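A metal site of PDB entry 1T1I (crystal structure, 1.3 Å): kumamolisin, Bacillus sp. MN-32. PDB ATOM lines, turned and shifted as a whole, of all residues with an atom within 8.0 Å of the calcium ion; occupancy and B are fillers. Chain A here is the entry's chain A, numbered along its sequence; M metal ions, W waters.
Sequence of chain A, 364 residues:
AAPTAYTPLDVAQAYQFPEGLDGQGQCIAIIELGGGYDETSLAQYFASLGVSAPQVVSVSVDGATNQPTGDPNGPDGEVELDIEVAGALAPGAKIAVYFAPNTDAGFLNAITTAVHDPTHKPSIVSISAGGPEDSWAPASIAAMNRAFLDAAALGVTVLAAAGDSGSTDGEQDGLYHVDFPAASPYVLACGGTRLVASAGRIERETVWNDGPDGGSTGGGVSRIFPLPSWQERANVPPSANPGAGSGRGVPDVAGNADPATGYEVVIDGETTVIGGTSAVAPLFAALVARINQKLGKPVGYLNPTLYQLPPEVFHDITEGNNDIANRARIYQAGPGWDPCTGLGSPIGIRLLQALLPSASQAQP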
ATOM      1  N   VAL A 207     -28.210 -27.443  21.779  1.00  0.00           N
ATOM      2  CA  VAL A 207     -29.423 -27.489  20.956  1.00  0.00           C
ATOM      3  C   VAL A 207     -29.852 -28.959  20.729  1.00  0.00           C
ATOM      4  O   VAL A 207     -29.006 -29.826  20.474  1.00  0.00           O
ATOM      5  CB  VAL A 207     -29.189 -26.868  19.532  1.00  0.00           C
ATOM      6  CG1 VAL A 207     -30.474 -26.976  18.699  1.00  0.00           C
ATOM      7  CG2 VAL A 207     -28.761 -25.399  19.651  1.00  0.00           C
ATOM      8  N   HIS A 315     -29.803 -19.164  31.272  1.00  0.00           N
ATOM      9  CA  HIS A 315     -28.639 -19.999  30.993  1.00  0.00           C
ATOM     10  C   HIS A 315     -28.552 -19.948  29.460  1.00  0.00           C
ATOM     11  O   HIS A 315     -29.400 -20.517  28.766  1.00  0.00           O
ATOM     12  CB  HIS A 315     -28.887 -21.426  31.465  1.00  0.00           C
ATOM     13  CG  HIS A 315     -27.782 -22.388  31.120  1.00  0.00           C
ATOM     14  ND1 HIS A 315     -26.669 -22.547  31.909  1.00  0.00           N
ATOM     15  CD2 HIS A 315     -27.617 -23.214  30.059  1.00  0.00           C
ATOM     16  CE1 HIS A 315     -25.863 -23.439  31.355  1.00  0.00           C
ATOM     17  NE2 HIS A 315     -26.420 -23.859  30.228  1.00  0.00           N
ATOM     18  N   ASP A 316     -27.537 -19.267  28.947  1.00  0.00           N
ATOM     19  CA  ASP A 316     -27.338 -19.119  27.506  1.00  0.00           C
ATOM     20  C   ASP A 316     -26.850 -20.422  26.825  1.00  0.00           C
ATOM     21  O   ASP A 316     -25.820 -20.969  27.203  1.00  0.00           O
ATOM     22  CB  ASP A 316     -26.308 -17.987  27.306  1.00  0.00           C
ATOM     23  CG  ASP A 316     -26.209 -17.515  25.874  1.00  0.00           C
ATOM     24  OD1 ASP A 316     -26.931 -18.070  25.033  1.00  0.00           O
ATOM     25  OD2 ASP A 316     -25.407 -16.603  25.573  1.00  0.00           O
ATOM     26  N   ILE A 317     -27.607 -20.936  25.849  1.00  0.00           N
ATOM     27  CA  ILE A 317     -27.148 -22.122  25.119  1.00  0.00           C
ATOM     28  C   ILE A 317     -26.382 -21.526  23.936  1.00  0.00           C
ATOM     29  O   ILE A 317     -26.907 -20.689  23.215  1.00  0.00           O
ATOM     30  CB  ILE A 317     -28.329 -23.023  24.603  1.00  0.00           C
ATOM     31  CG1 ILE A 317     -28.896 -23.874  25.756  1.00  0.00           C
ATOM     32  CG2 ILE A 317     -27.821 -24.012  23.567  1.00  0.00           C
ATOM     33  CD1 ILE A 317     -29.751 -23.160  26.746  1.00  0.00           C
ATOM     34  N   THR A 318     -25.144 -21.956  23.720  1.00  0.00           N
ATOM     35  CA  THR A 318     -24.349 -21.368  22.645  1.00  0.00           C
ATOM     36  C   THR A 318     -23.843 -22.371  21.610  1.00  0.00           C
ATOM     37  O   THR A 318     -23.225 -21.987  20.623  1.00  0.00           O
ATOM     38  CB  THR A 318     -23.106 -20.677  23.231  1.00  0.00           C
ATOM     39  OG1 THR A 318     -22.319 -21.648  23.938  1.00  0.00           O
ATOM     40  CG2 THR A 318     -23.500 -19.562  24.194  1.00  0.00           C
ATOM     41  N   GLU A 319     -24.105 -23.652  21.840  1.00  0.00           N
ATOM     42  CA  GLU A 319     -23.611 -24.697  20.964  1.00  0.00           C
ATOM     43  C   GLU A 319     -24.695 -25.579  20.313  1.00  0.00           C
ATOM     44  O   GLU A 319     -25.631 -26.015  20.980  1.00  0.00           O
ATOM     45  CB  GLU A 319     -22.612 -25.540  21.764  1.00  0.00           C
ATOM     46  CG  GLU A 319     -22.149 -26.824  21.110  1.00  0.00           C
ATOM     47  CD  GLU A 319     -21.061 -27.531  21.908  1.00  0.00           C
ATOM     48  OE1 GLU A 319     -20.986 -27.304  23.150  1.00  0.00           O
ATOM     49  OE2 GLU A 319     -20.295 -28.307  21.296  1.00  0.00           O
ATOM     50  N   GLN A 332     -28.144 -21.660  13.718  1.00  0.00           N
ATOM     51  CA  GLN A 332     -27.109 -21.976  14.672  1.00  0.00           C
ATOM     52  C   GLN A 332     -27.236 -21.230  15.997  1.00  0.00           C
ATOM     53  O   GLN A 332     -27.654 -20.064  16.042  1.00  0.00           O
ATOM     54  CB  GLN A 332     -25.774 -21.659  14.016  1.00  0.00           C
ATOM     55  CG  GLN A 332     -24.586 -22.270  14.680  1.00  0.00           C
ATOM     56  CD  GLN A 332     -23.422 -22.378  13.718  1.00  0.00           C
ATOM     57  OE1 GLN A 332     -22.994 -21.387  13.141  1.00  0.00           O
ATOM     58  NE2 GLN A 332     -22.926 -23.585  13.521  1.00  0.00           N
ATOM     59  N   ALA A 333     -26.875 -21.902  17.092  1.00  0.00           N
ATOM     60  CA  ALA A 333     -26.935 -21.310  18.425  1.00  0.00           C
ATOM     61  C   ALA A 333     -25.647 -20.488  18.594  1.00  0.00           C
ATOM     62  O   ALA A 333     -24.672 -20.697  17.889  1.00  0.00           O
ATOM     63  CB  ALA A 333     -27.001 -22.386  19.497  1.00  0.00           C
ATOM     64  N   GLY A 334     -25.663 -19.548  19.519  1.00  0.00           N
ATOM     65  CA  GLY A 334     -24.479 -18.733  19.733  1.00  0.00           C
ATOM     66  C   GLY A 334     -24.713 -17.854  20.936  1.00  0.00           C
ATOM     67  O   GLY A 334     -25.731 -17.976  21.603  1.00  0.00           O
ATOM     68  N   PRO A 335     -23.775 -16.956  21.267  1.00  0.00           N
ATOM     69  CA  PRO A 335     -23.947 -16.079  22.432  1.00  0.00           C
ATOM     70  C   PRO A 335     -25.198 -15.197  22.289  1.00  0.00           C
ATOM     71  O   PRO A 335     -25.475 -14.656  21.213  1.00  0.00           O
ATOM     72  CB  PRO A 335     -22.638 -15.279  22.448  1.00  0.00           C
ATOM     73  CG  PRO A 335     -22.251 -15.240  20.979  1.00  0.00           C
ATOM     74  CD  PRO A 335     -22.541 -16.651  20.525  1.00  0.00           C
ATOM     75  N   GLY A 336     -25.961 -15.048  23.380  1.00  0.00           N
ATOM     76  CA  GLY A 336     -27.165 -14.238  23.360  1.00  0.00           C
ATOM     77  C   GLY A 336     -28.353 -14.976  22.724  1.00  0.00           C
ATOM     78  O   GLY A 336     -28.320 -16.183  22.553  1.00  0.00           O
ATOM     79  N   TRP A 337     -29.404 -14.253  22.359  1.00  0.00           N
ATOM     80  CA  TRP A 337     -30.558 -14.870  21.730  1.00  0.00           C
ATOM     81  C   TRP A 337     -30.169 -15.529  20.388  1.00  0.00           C
ATOM     82  O   TRP A 337     -29.337 -14.980  19.662  1.00  0.00           O
ATOM     83  CB  TRP A 337     -31.635 -13.795  21.472  1.00  0.00           C
ATOM     84  CG  TRP A 337     -32.939 -14.324  20.935  1.00  0.00           C
ATOM     85  CD1 TRP A 337     -34.065 -14.610  21.661  1.00  0.00           C
ATOM     86  CD2 TRP A 337     -33.222 -14.753  19.578  1.00  0.00           C
ATOM     87  NE1 TRP A 337     -35.014 -15.209  20.858  1.00  0.00           N
ATOM     88  CE2 TRP A 337     -34.531 -15.300  19.579  1.00  0.00           C
ATOM     89  CE3 TRP A 337     -32.490 -14.723  18.372  1.00  0.00           C
ATOM     90  CZ2 TRP A 337     -35.131 -15.836  18.423  1.00  0.00           C
ATOM     91  CZ3 TRP A 337     -33.085 -15.252  17.219  1.00  0.00           C
ATOM     92  CH2 TRP A 337     -34.391 -15.802  17.249  1.00  0.00           C
ATOM     93  N   ASP A 338     -30.731 -16.706  20.093  1.00  0.00           N
ATOM     94  CA  ASP A 338     -30.505 -17.383  18.801  1.00  0.00           C
ATOM     95  C   ASP A 338     -31.804 -18.094  18.345  1.00  0.00           C
ATOM     96  O   ASP A 338     -32.719 -18.312  19.148  1.00  0.00           O
ATOM     97  CB  ASP A 338     -29.316 -18.349  18.825  1.00  0.00           C
ATOM     98  CG  ASP A 338     -29.425 -19.418  19.872  1.00  0.00           C
ATOM     99  OD1 ASP A 338     -30.329 -20.285  19.780  1.00  0.00           O
ATOM    100  OD2 ASP A 338     -28.591 -19.409  20.800  1.00  0.00           O
ATOM    101  N   PRO A 339     -31.913 -18.428  17.041  1.00  0.00           N
ATOM    102  CA  PRO A 339     -33.108 -19.086  16.505  1.00  0.00           C
ATOM    103  C   PRO A 339     -33.238 -20.589  16.747  1.00  0.00           C
ATOM    104  O   PRO A 339     -33.926 -21.282  16.016  1.00  0.00           O
ATOM    105  CB  PRO A 339     -33.066 -18.750  14.996  1.00  0.00           C
ATOM    106  CG  PRO A 339     -31.841 -17.829  14.821  1.00  0.00           C
ATOM    107  CD  PRO A 339     -30.939 -18.188  15.964  1.00  0.00           C
ATOM    108  N   CYS A 340     -32.558 -21.094  17.765  1.00  0.00           N
ATOM    109  CA  CYS A 340     -32.656 -22.501  18.149  1.00  0.00           C
ATOM    110  C   CYS A 340     -33.211 -22.568  19.586  1.00  0.00           C
ATOM    111  O   CYS A 340     -34.061 -23.413  19.885  1.00  0.00           O
ATOM    112  CB  CYS A 340     -31.271 -23.181  18.167  1.00  0.00           C
ATOM    113  SG  CYS A 340     -30.366 -23.188  16.622  1.00  0.00           S
ATOM    114  N   THR A 341     -32.733 -21.658  20.439  1.00  0.00           N
ATOM    115  CA  THR A 341     -33.073 -21.680  21.852  1.00  0.00           C
ATOM    116  C   THR A 341     -33.519 -20.352  22.471  1.00  0.00           C
ATOM    117  O   THR A 341     -33.782 -20.293  23.681  1.00  0.00           O
ATOM    118  CB  THR A 341     -31.854 -22.217  22.649  1.00  0.00           C
ATOM    119  OG1 THR A 341     -30.710 -21.374  22.432  1.00  0.00           O
ATOM    120  CG2 THR A 341     -31.506 -23.644  22.192  1.00  0.00           C
ATOM    121  N   GLY A 342     -33.616 -19.315  21.654  1.00  0.00           N
ATOM    122  CA  GLY A 342     -34.025 -18.025  22.180  1.00  0.00           C
ATOM    123  C   GLY A 342     -33.073 -17.505  23.243  1.00  0.00           C
ATOM    124  O   GLY A 342     -31.864 -17.542  23.058  1.00  0.00           O
ATOM    125  N   LEU A 343     -33.611 -17.025  24.356  1.00  0.00           N
ATOM    126  CA  LEU A 343     -32.813 -16.496  25.458  1.00  0.00           C
ATOM    127  C   LEU A 343     -32.108 -17.590  26.267  1.00  0.00           C
ATOM    128  O   LEU A 343     -31.230 -17.299  27.084  1.00  0.00           O
ATOM    129  CB  LEU A 343     -33.713 -15.659  26.384  1.00  0.00           C
ATOM    130  CG  LEU A 343     -34.387 -14.446  25.726  1.00  0.00           C
ATOM    131  CD1 LEU A 343     -35.388 -13.806  26.684  1.00  0.00           C
ATOM    132  CD2 LEU A 343     -33.312 -13.456  25.298  1.00  0.00           C
ATOM    133  N   GLY A 344     -32.486 -18.838  26.012  1.00  0.00           N
ATOM    134  CA  GLY A 344     -31.881 -19.971  26.701  1.00  0.00           C
ATOM    135  C   GLY A 344     -32.845 -20.594  27.703  1.00  0.00           C
ATOM    136  O   GLY A 344     -34.058 -20.393  27.623  1.00  0.00           O
ATOM    137  N   SER A 345     -32.317 -21.378  28.645  1.00  0.00           N
ATOM    138  CA  SER A 345     -33.204 -21.978  29.643  1.00  0.00           C
ATOM    139  C   SER A 345     -33.264 -21.012  30.834  1.00  0.00           C
ATOM    140  O   SER A 345     -32.256 -20.456  31.267  1.00  0.00           O
ATOM    141  CB  SER A 345     -32.684 -23.365  30.067  1.00  0.00           C
ATOM    142  OG  SER A 345     -31.343 -23.346  30.549  1.00  0.00           O
HETATM  143 CA    CA M   1     -27.733 -18.445  22.834  1.00  0.00          CA
HETATM  144  O   HOH W   1     -29.882 -19.196  23.874  1.00  0.00           O
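The backbone NH (N) of Thr 341 sits at hydrogen-bond distance from the side-chain carboxylate (OD1) of Asp 338. The side-chain carboxylate (OD1) of Asp 338 lies within hydrogen-bond range of the backbone NH (N) of Cys 340 (3.1 Å).
Five residues have an atom within 4 Å of the calcium ion: Asp 316, Ile 317, Gly 334, Gly 336 and Asp 338.
The calcium ion is bound by O of Gly 336 (2.4 Å), OD1 of Asp 316 (2.4 Å), O of Gly 334 (2.4 Å), OD2 of Asp 338 (2.4 Å), O of Ile 317 (2.4 Å) and water W1 (2.5 Å). The calcium ion has six donor atoms within binding distance.
Water W1 lies within hydrogen-bond range of the backbone carbonyl oxygen of Gly 342 (2.7 Å), the side-chain hydroxyl of Thr 341 (2.7 Å), the backbone NH of Gly 344 (3.4 Å) and the backbone NH of Ile 317 (3.5 Å).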
